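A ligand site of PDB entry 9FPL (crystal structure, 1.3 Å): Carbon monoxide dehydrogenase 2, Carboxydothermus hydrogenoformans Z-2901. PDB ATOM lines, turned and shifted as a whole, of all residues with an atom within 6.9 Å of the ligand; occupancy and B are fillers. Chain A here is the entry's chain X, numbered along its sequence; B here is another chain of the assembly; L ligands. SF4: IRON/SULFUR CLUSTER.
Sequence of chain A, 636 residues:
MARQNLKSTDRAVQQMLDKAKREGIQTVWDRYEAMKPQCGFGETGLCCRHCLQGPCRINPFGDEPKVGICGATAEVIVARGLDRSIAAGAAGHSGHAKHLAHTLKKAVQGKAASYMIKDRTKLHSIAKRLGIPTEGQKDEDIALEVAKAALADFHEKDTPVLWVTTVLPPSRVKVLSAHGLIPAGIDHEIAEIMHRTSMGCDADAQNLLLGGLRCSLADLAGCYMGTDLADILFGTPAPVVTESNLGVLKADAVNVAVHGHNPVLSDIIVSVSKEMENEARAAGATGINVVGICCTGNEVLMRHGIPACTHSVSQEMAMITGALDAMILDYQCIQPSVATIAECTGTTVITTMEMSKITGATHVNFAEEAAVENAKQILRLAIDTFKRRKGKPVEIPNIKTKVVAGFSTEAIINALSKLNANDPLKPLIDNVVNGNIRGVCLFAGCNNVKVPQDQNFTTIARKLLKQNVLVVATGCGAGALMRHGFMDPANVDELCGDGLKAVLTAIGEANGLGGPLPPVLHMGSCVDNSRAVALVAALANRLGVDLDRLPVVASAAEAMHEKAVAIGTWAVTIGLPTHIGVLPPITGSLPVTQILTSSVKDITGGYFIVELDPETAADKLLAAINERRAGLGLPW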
ATOM      1  N   CYS A  47      10.020  15.694  -7.876  1.00  0.00           N
ATOM      2  CA  CYS A  47      10.235  15.799  -6.436  1.00  0.00           C
ATOM      3  C   CYS A  47       9.194  16.774  -5.899  1.00  0.00           C
ATOM      4  O   CYS A  47       8.897  17.776  -6.551  1.00  0.00           O
ATOM      5  CB  CYS A  47      11.629  16.294  -6.049  1.00  0.00           C
ATOM      6  SG  CYS A  47      11.870  16.521  -4.261  1.00  0.00           S
ATOM      7  N   CYS A  48       8.638  16.466  -4.737  1.00  0.00           N
ATOM      8  CA  CYS A  48       7.675  17.346  -4.093  1.00  0.00           C
ATOM      9  C   CYS A  48       7.988  17.424  -2.608  1.00  0.00           C
ATOM     10  O   CYS A  48       8.195  16.392  -1.951  1.00  0.00           O
ATOM     11  CB  CYS A  48       6.270  16.799  -4.269  1.00  0.00           C
ATOM     12  SG  CYS A  48       5.007  17.836  -3.481  1.00  0.00           S
ATOM     13  N   ARG A  49       8.031  18.660  -2.098  1.00  0.00           N
ATOM     14  CA  ARG A  49       8.193  18.964  -0.686  1.00  0.00           C
ATOM     15  C   ARG A  49       7.051  19.838  -0.183  1.00  0.00           C
ATOM     16  O   ARG A  49       7.222  20.655   0.734  1.00  0.00           O
ATOM     17  CB  ARG A  49       9.547  19.633  -0.429  1.00  0.00           C
ATOM     18  CG  ARG A  49      10.674  18.692  -0.760  1.00  0.00           C
ATOM     19  CD  ARG A  49      12.015  19.423  -0.793  1.00  0.00           C
ATOM     20  NE  ARG A  49      12.300  19.988   0.511  1.00  0.00           N
ATOM     21  CZ  ARG A  49      13.042  21.047   0.757  1.00  0.00           C
ATOM     22  NH1 ARG A  49      13.702  21.680  -0.182  1.00  0.00           N
ATOM     23  NH2 ARG A  49      13.181  21.452   2.028  1.00  0.00           N
ATOM     24  N   HIS A  50       5.863  19.670  -0.763  1.00  0.00           N
ATOM     25  CA  HIS A  50       4.748  20.532  -0.391  1.00  0.00           C
ATOM     26  C   HIS A  50       4.060  20.143   0.908  1.00  0.00           C
ATOM     27  O   HIS A  50       3.143  20.865   1.330  1.00  0.00           O
ATOM     28  CB  HIS A  50       3.739  20.667  -1.513  1.00  0.00           C
ATOM     29  CG  HIS A  50       4.261  21.380  -2.725  1.00  0.00           C
ATOM     30  ND1 HIS A  50       3.453  21.890  -3.699  1.00  0.00           N
ATOM     31  CD2 HIS A  50       5.535  21.645  -3.112  1.00  0.00           C
ATOM     32  CE1 HIS A  50       4.199  22.425  -4.662  1.00  0.00           C
ATOM     33  NE2 HIS A  50       5.479  22.307  -4.325  1.00  0.00           N
ATOM     34  N   CYS A  51       4.494  19.094   1.583  1.00  0.00           N
ATOM     35  CA  CYS A  51       3.996  18.823   2.932  1.00  0.00           C
ATOM     36  C   CYS A  51       5.021  18.031   3.727  1.00  0.00           C
ATOM     37  O   CYS A  51       6.034  17.588   3.178  1.00  0.00           O
ATOM     38  CB  CYS A  51       2.620  18.153   2.956  1.00  0.00           C
ATOM     39  SG  CYS A  51       2.649  16.347   2.727  1.00  0.00           S
ATOM     40  N   LEU A  52       4.773  17.890   5.022  1.00  0.00           N
ATOM     41  CA  LEU A  52       5.719  17.260   5.929  1.00  0.00           C
ATOM     42  C   LEU A  52       5.657  15.756   5.902  1.00  0.00           C
ATOM     43  O   LEU A  52       6.401  15.116   6.670  1.00  0.00           O
ATOM     44  CB  LEU A  52       5.546  17.774   7.366  1.00  0.00           C
ATOM     45  CG  LEU A  52       5.668  19.294   7.530  1.00  0.00           C
ATOM     46  CD1 LEU A  52       5.462  19.720   8.990  1.00  0.00           C
ATOM     47  CD2 LEU A  52       7.010  19.777   7.049  1.00  0.00           C
ATOM     48  N   GLN A  53       4.841  15.176   5.016  1.00  0.00           N
ATOM     49  CA  GLN A  53       4.977  13.769   4.698  1.00  0.00           C
ATOM     50  C   GLN A  53       6.125  13.530   3.740  1.00  0.00           C
ATOM     51  O   GLN A  53       6.601  12.386   3.644  1.00  0.00           O
ATOM     52  CB  GLN A  53       3.675  13.160   4.168  1.00  0.00           C
ATOM     53  CG  GLN A  53       2.652  13.063   5.272  1.00  0.00           C
ATOM     54  CD  GLN A  53       1.308  12.519   4.873  1.00  0.00           C
ATOM     55  OE1 GLN A  53       0.547  12.076   5.715  1.00  0.00           O
ATOM     56  NE2 GLN A  53       1.010  12.534   3.586  1.00  0.00           N
ATOM     57  N   GLY A  54       6.561  14.574   3.031  1.00  0.00           N
ATOM     58  CA  GLY A  54       7.637  14.431   2.086  1.00  0.00           C
ATOM     59  C   GLY A  54       8.970  14.417   2.779  1.00  0.00           C
ATOM     60  O   GLY A  54       9.077  14.383   4.006  1.00  0.00           O
ATOM     61  N   PRO A  55      10.031  14.470   1.994  1.00  0.00           N
ATOM     62  CA  PRO A  55      10.043  14.663   0.560  1.00  0.00           C
ATOM     63  C   PRO A  55       9.574  13.425  -0.179  1.00  0.00           C
ATOM     64  O   PRO A  55       9.902  12.293   0.173  1.00  0.00           O
ATOM     65  CB  PRO A  55      11.536  14.978   0.262  1.00  0.00           C
ATOM     66  CG  PRO A  55      12.263  14.252   1.342  1.00  0.00           C
ATOM     67  CD  PRO A  55      11.383  14.323   2.557  1.00  0.00           C
ATOM     68  N   CYS A  56       8.847  13.673  -1.255  1.00  0.00           N
ATOM     69  CA  CYS A  56       8.398  12.657  -2.187  1.00  0.00           C
ATOM     70  C   CYS A  56       9.144  12.789  -3.497  1.00  0.00           C
ATOM     71  O   CYS A  56       9.515  13.889  -3.924  1.00  0.00           O
ATOM     72  CB  CYS A  56       6.895  12.779  -2.432  1.00  0.00           C
ATOM     73  SG  CYS A  56       5.902  12.254  -1.006  1.00  0.00           S
ATOM     74  N   ARG A  57       9.314  11.658  -4.169  1.00  0.00           N
ATOM     75  CA  ARG A  57       9.969  11.645  -5.474  1.00  0.00           C
ATOM     76  C   ARG A  57       9.321  10.537  -6.275  1.00  0.00           C
ATOM     77  O   ARG A  57       8.656   9.649  -5.734  1.00  0.00           O
ATOM     78  CB  ARG A  57      11.476  11.429  -5.328  1.00  0.00           C
ATOM     79  CG  ARG A  57      11.807  10.034  -4.915  1.00  0.00           C
ATOM     80  CD  ARG A  57      13.244   9.890  -4.357  1.00  0.00           C
ATOM     81  NE  ARG A  57      13.521   8.494  -4.041  1.00  0.00           N
ATOM     82  CZ  ARG A  57      12.976   7.846  -3.018  1.00  0.00           C
ATOM     83  NH1 ARG A  57      12.316   8.469  -2.047  1.00  0.00           N
ATOM     84  NH2 ARG A  57      13.077   6.513  -2.964  1.00  0.00           N
ATOM     85  N   VAL A  67       4.417   7.245  -7.396  1.00  0.00           N
ATOM     86  CA  VAL A  67       3.396   8.229  -7.070  1.00  0.00           C
ATOM     87  C   VAL A  67       3.755   8.799  -5.710  1.00  0.00           C
ATOM     88  O   VAL A  67       4.408   8.151  -4.898  1.00  0.00           O
ATOM     89  CB  VAL A  67       2.021   7.537  -7.106  1.00  0.00           C
ATOM     90  CG1 VAL A  67       1.971   6.423  -6.085  1.00  0.00           C
ATOM     91  CG2 VAL A  67       0.928   8.522  -6.917  1.00  0.00           C
ATOM     92  N   GLY A  68       3.335  10.043  -5.477  1.00  0.00           N
ATOM     93  CA  GLY A  68       3.571  10.685  -4.212  1.00  0.00           C
ATOM     94  C   GLY A  68       2.759  10.031  -3.105  1.00  0.00           C
ATOM     95  O   GLY A  68       1.781   9.333  -3.341  1.00  0.00           O
ATOM     96  N   ILE A  69       3.156  10.294  -1.875  1.00  0.00           N
ATOM     97  CA  ILE A  69       2.520   9.661  -0.717  1.00  0.00           C
ATOM     98  C   ILE A  69       1.018   9.950  -0.683  1.00  0.00           C
ATOM     99  O   ILE A  69       0.205   9.057  -0.375  1.00  0.00           O
ATOM    100  CB  ILE A  69       3.252  10.050   0.575  1.00  0.00           C
ATOM    101  CG1 ILE A  69       4.612   9.324   0.601  1.00  0.00           C
ATOM    102  CG2 ILE A  69       2.403   9.667   1.792  1.00  0.00           C
ATOM    103  CD1 ILE A  69       5.539   9.756   1.682  1.00  0.00           C
ATOM    104  N   CYS A  70       0.605  11.215  -0.941  1.00  0.00           N
ATOM    105  CA  CYS A  70      -0.827  11.558  -0.940  1.00  0.00           C
ATOM    106  C   CYS A  70      -1.575  11.079  -2.181  1.00  0.00           C
ATOM    107  O   CYS A  70      -2.798  11.257  -2.260  1.00  0.00           O
ATOM    108  CB  CYS A  70      -0.959  13.076  -0.844  1.00  0.00           C
ATOM    109  SG  CYS A  70      -0.204  13.897  -2.269  1.00  0.00           S
ATOM    110  N   GLY A  71      -0.862  10.484  -3.154  1.00  0.00           N
ATOM    111  CA  GLY A  71      -1.442  10.096  -4.424  1.00  0.00           C
ATOM    112  C   GLY A  71      -1.110  11.013  -5.569  1.00  0.00           C
ATOM    113  O   GLY A  71      -1.558  10.759  -6.696  1.00  0.00           O
ATOM    114  N   ALA A  72      -0.354  12.071  -5.314  1.00  0.00           N
ATOM    115  CA  ALA A  72      -0.014  13.016  -6.388  1.00  0.00           C
ATOM    116  C   ALA A  72       0.800  12.314  -7.476  1.00  0.00           C
ATOM    117  O   ALA A  72       1.855  11.725  -7.216  1.00  0.00           O
ATOM    118  CB  ALA A  72       0.777  14.166  -5.815  1.00  0.00           C
ATOM    119  N   THR A  73       0.324  12.418  -8.715  1.00  0.00           N
ATOM    120  CA  THR A  73       0.984  11.800  -9.845  1.00  0.00           C
ATOM    121  C   THR A  73       2.170  12.654 -10.312  1.00  0.00           C
ATOM    122  O   THR A  73       2.347  13.806  -9.898  1.00  0.00           O
ATOM    123  CB  THR A  73       0.021  11.658 -11.007  1.00  0.00           C
ATOM    124  OG1 THR A  73      -0.424  12.976 -11.354  1.00  0.00           O
ATOM    125  CG2 THR A  73      -1.186  10.755 -10.690  1.00  0.00           C
ATOM    126  N   ILE A  77       2.666  16.670  -9.713  1.00  0.00           N
ATOM    127  CA  ILE A  77       3.875  17.179  -9.066  1.00  0.00           C
ATOM    128  C   ILE A  77       4.604  18.153  -9.991  1.00  0.00           C
ATOM    129  O   ILE A  77       4.983  19.270  -9.587  1.00  0.00           O
ATOM    130  CB  ILE A  77       4.781  16.006  -8.634  1.00  0.00           C
ATOM    131  CG1 ILE A  77       4.145  15.345  -7.406  1.00  0.00           C
ATOM    132  CG2 ILE A  77       6.181  16.471  -8.328  1.00  0.00           C
ATOM    133  CD1 ILE A  77       4.806  14.049  -6.960  1.00  0.00           C
ATOM    134  N   ARG A  80       2.521  21.433 -10.408  1.00  0.00           N
ATOM    135  CA  ARG A  80       2.536  22.260  -9.202  1.00  0.00           C
ATOM    136  C   ARG A  80       3.859  22.983  -9.004  1.00  0.00           C
ATOM    137  O   ARG A  80       3.879  24.156  -8.642  1.00  0.00           O
ATOM    138  CB  ARG A  80       2.235  21.426  -7.960  1.00  0.00           C
ATOM    139  CG  ARG A  80       0.796  20.921  -7.924  1.00  0.00           C
ATOM    140  CD  ARG A  80       0.351  20.264  -6.605  1.00  0.00           C
ATOM    141  NE  ARG A  80       1.264  19.234  -6.124  1.00  0.00           N
ATOM    142  CZ  ARG A  80       0.954  18.426  -5.132  1.00  0.00           C
ATOM    143  NH1 ARG A  80      -0.234  18.472  -4.571  1.00  0.00           N
ATOM    144  NH2 ARG A  80       1.847  17.533  -4.710  1.00  0.00           N
ATOM    145  N   THR A 197      -1.690  24.831  -5.380  1.00  0.00           N
ATOM    146  CA  THR A 197      -0.575  23.909  -5.451  1.00  0.00           C
ATOM    147  C   THR A 197      -0.194  23.326  -4.094  1.00  0.00           C
ATOM    148  O   THR A 197       0.698  22.457  -4.034  1.00  0.00           O
ATOM    149  CB  THR A 197       0.651  24.584  -6.058  1.00  0.00           C
ATOM    150  OG1 THR A 197       1.015  25.716  -5.263  1.00  0.00           O
ATOM    151  CG2 THR A 197       0.425  24.987  -7.521  1.00  0.00           C
ATOM    152  N   SER A 198      -0.807  23.780  -3.015  1.00  0.00           N
ATOM    153  CA  SER A 198      -0.595  23.184  -1.710  1.00  0.00           C
ATOM    154  C   SER A 198      -1.245  21.795  -1.658  1.00  0.00           C
ATOM    155  O   SER A 198      -2.019  21.410  -2.527  1.00  0.00           O
ATOM    156  CB  SER A 198      -1.092  24.115  -0.610  1.00  0.00           C
ATOM    157  OG  SER A 198      -2.488  24.142  -0.449  1.00  0.00           O
ATOM    158  N   MET A 199      -0.901  21.056  -0.619  1.00  0.00           N
ATOM    159  CA  MET A 199      -1.289  19.653  -0.580  1.00  0.00           C
ATOM    160  C   MET A 199      -2.808  19.516  -0.572  1.00  0.00           C
ATOM    161  O   MET A 199      -3.538  20.245   0.131  1.00  0.00           O
ATOM    162  CB  MET A 199      -0.683  18.982   0.655  1.00  0.00           C
ATOM    163  CG  MET A 199      -1.005  17.500   0.812  1.00  0.00           C
ATOM    164  SD  MET A 199      -2.656  17.240   1.498  1.00  0.00           S
ATOM    165  CE  MET A 199      -3.156  15.691   0.712  1.00  0.00           C
ATOM    166  N   GLY A 200      -3.299  18.552  -1.362  1.00  0.00           N
ATOM    167  CA  GLY A 200      -4.699  18.177  -1.329  1.00  0.00           C
ATOM    168  C   GLY A 200      -5.617  19.171  -1.960  1.00  0.00           C
ATOM    169  O   GLY A 200      -6.819  19.202  -1.648  1.00  0.00           O
ATOM    170  N   VAL B  28      -2.421   5.241   1.485  1.00  0.00           N
ATOM    171  CA  VAL B  28      -1.373   6.203   1.836  1.00  0.00           C
ATOM    172  C   VAL B  28      -0.208   5.520   2.553  1.00  0.00           C
ATOM    173  O   VAL B  28       0.952   5.868   2.371  1.00  0.00           O
ATOM    174  CB  VAL B  28      -1.997   7.348   2.681  1.00  0.00           C
ATOM    175  CG1 VAL B  28      -2.556   6.842   4.025  1.00  0.00           C
ATOM    176  CG2 VAL B  28      -1.006   8.473   2.864  1.00  0.00           C
ATOM    177  N   MET B  35       8.022   4.821  -0.714  1.00  0.00           N
ATOM    178  CA  MET B  35       8.853   6.021  -0.794  1.00  0.00           C
ATOM    179  C   MET B  35      10.121   5.904   0.034  1.00  0.00           C
ATOM    180  O   MET B  35      11.022   6.744  -0.088  1.00  0.00           O
ATOM    181  CB  MET B  35       8.040   7.236  -0.340  1.00  0.00           C
ATOM    182  CG  MET B  35       8.604   8.559  -0.798  1.00  0.00           C
ATOM    183  SD  MET B  35       8.641   8.795  -2.564  1.00  0.00           S
ATOM    184  CE  MET B  35       6.928   8.777  -3.058  1.00  0.00           C
ATOM    185  N   GLN B  38      13.360   8.030   2.309  1.00  0.00           N
ATOM    186  CA  GLN B  38      13.148   9.357   1.750  1.00  0.00           C
ATOM    187  C   GLN B  38      14.466  10.135   1.708  1.00  0.00           C
ATOM    188  O   GLN B  38      15.431   9.829   2.422  1.00  0.00           O
ATOM    189  CB  GLN B  38      12.083  10.118   2.550  1.00  0.00           C
ATOM    190  CG  GLN B  38      10.727   9.507   2.382  1.00  0.00           C
ATOM    191  CD  GLN B  38       9.675  10.125   3.243  1.00  0.00           C
ATOM    192  OE1 GLN B  38       9.564   9.813   4.432  1.00  0.00           O
ATOM    193  NE2 GLN B  38       8.872  11.003   2.657  1.00  0.00           N
ATOM    194  N   PRO B 336      -5.321  13.045  -3.426  1.00  0.00           N
ATOM    195  CA  PRO B 336      -5.883  12.825  -4.768  1.00  0.00           C
ATOM    196  C   PRO B 336      -6.041  11.371  -5.131  1.00  0.00           C
ATOM    197  O   PRO B 336      -6.735  11.038  -6.105  1.00  0.00           O
ATOM    198  CB  PRO B 336      -4.926  13.582  -5.692  1.00  0.00           C
ATOM    199  CG  PRO B 336      -3.658  13.642  -4.926  1.00  0.00           C
ATOM    200  CD  PRO B 336      -4.080  13.840  -3.484  1.00  0.00           C
ATOM    201  N   MET B 560       1.281  17.990   9.213  1.00  0.00           N
ATOM    202  CA  MET B 560       1.500  17.649   7.813  1.00  0.00           C
ATOM    203  C   MET B 560       1.476  18.830   6.835  1.00  0.00           C
ATOM    204  O   MET B 560       2.444  19.075   6.093  1.00  0.00           O
ATOM    205  CB  MET B 560       0.438  16.602   7.403  1.00  0.00           C
ATOM    206  CG  MET B 560       0.519  16.094   5.980  1.00  0.00           C
ATOM    207  SD  MET B 560      -0.485  17.027   4.784  1.00  0.00           S
ATOM    208  CE  MET B 560      -2.154  16.782   5.380  1.00  0.00           C
HETATM  209 FE1  SF4 L   1       4.381  14.010  -0.890  1.00  0.00          FE
HETATM  210 FE2  SF4 L   1       3.157  15.936   0.561  1.00  0.00          FE
HETATM  211 FE3  SF4 L   1       3.993  16.402  -1.998  1.00  0.00          FE
HETATM  212 FE4  SF4 L   1       1.858  14.740  -1.608  1.00  0.00          FE
HETATM  213  S1  SF4 L   1       2.031  17.007  -1.162  1.00  0.00           S
HETATM  214  S2  SF4 L   1       3.561  14.420  -2.984  1.00  0.00           S
HETATM  215  S3  SF4 L   1       2.567  13.722   0.335  1.00  0.00           S
HETATM  216  S4  SF4 L   1       5.300  15.993  -0.179  1.00  0.00           S
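Merely in contact with the ligand: Gly 68 (3.9 Å), Ile 69 (3.7 Å), Ala 72 (3.98 Å) and Met 199 (3.7 Å).
Within 4 Å of the ligand: Cys 48, His 50, Cys 51, Gln 53, Gly 54, Cys 56, Gly 68, Ile 69, Cys 70, Ala 72, Arg 80 and Met 199.
The nearest printed residue that does not touch the ligand is Arg 49 (4.2 Å).
The side-chain sulfur of Cys 51 sits close to the backbone NH of Gln 53.
The backbone carbonyl oxygen (O) of Cys 56 lies within hydrogen-bond range of the backbone NH (N) of Cys 48 (2.8 Å).
NH2 of Arg 80 sits close to SG of Cys 48 (3.4 Å).
The side-chain sulfur of Cys 48 sits close to the backbone NH of His 50 (3.4 Å).
The side-chain sulfur of Cys 70 sits close to the backbone NH of Ala 72, 3.6 Å away.
The backbone carbonyl oxygen of Cys 56 lies close to the side-chain sulfur of Cys 47 (3.5 Å).
A ring nitrogen (ND1) of His 50 sits at hydrogen-bond distance from the backbone carbonyl oxygen of Thr 197 (2.8 Å).
The side-chain amide nitrogen (NE2) of Gln 38 of chain B sits at hydrogen-bond distance from the backbone carbonyl oxygen (O) of Gln 53, at 2.8 Å.
The backbone NH (N) of Cys 51 lies close to a sulfur (S4) of the ligand.
SG of Cys 51 is bound to FE2 of the ligand (2.3 Å).
FE3 of the ligand is bound by SG of Cys 48 (2.3 Å).
A sulfur (S3) of the ligand lies close to the backbone NH of Cys 70, at 3.4 Å.
The side-chain sulfur of Cys 70 binds an iron atom (FE4) of the ligand (2.3 Å).
The side-chain sulfur (SG) of Cys 56 is bound to an iron atom (FE1) of the ligand (2.3 Å).
A sulfur (S1) of the ligand lies close to the guanidinium group (NH2) of Arg 80 (3.6 Å).
N of Gly 54 lies close to S4 of the ligand, 3.7 Å away.
N of His 50 sits close to S4 of the ligand (3.8 Å).
A sulfur (S3) of the ligand lies close to the side-chain amide nitrogen (NE2) of Gln 53 (3.8 Å).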
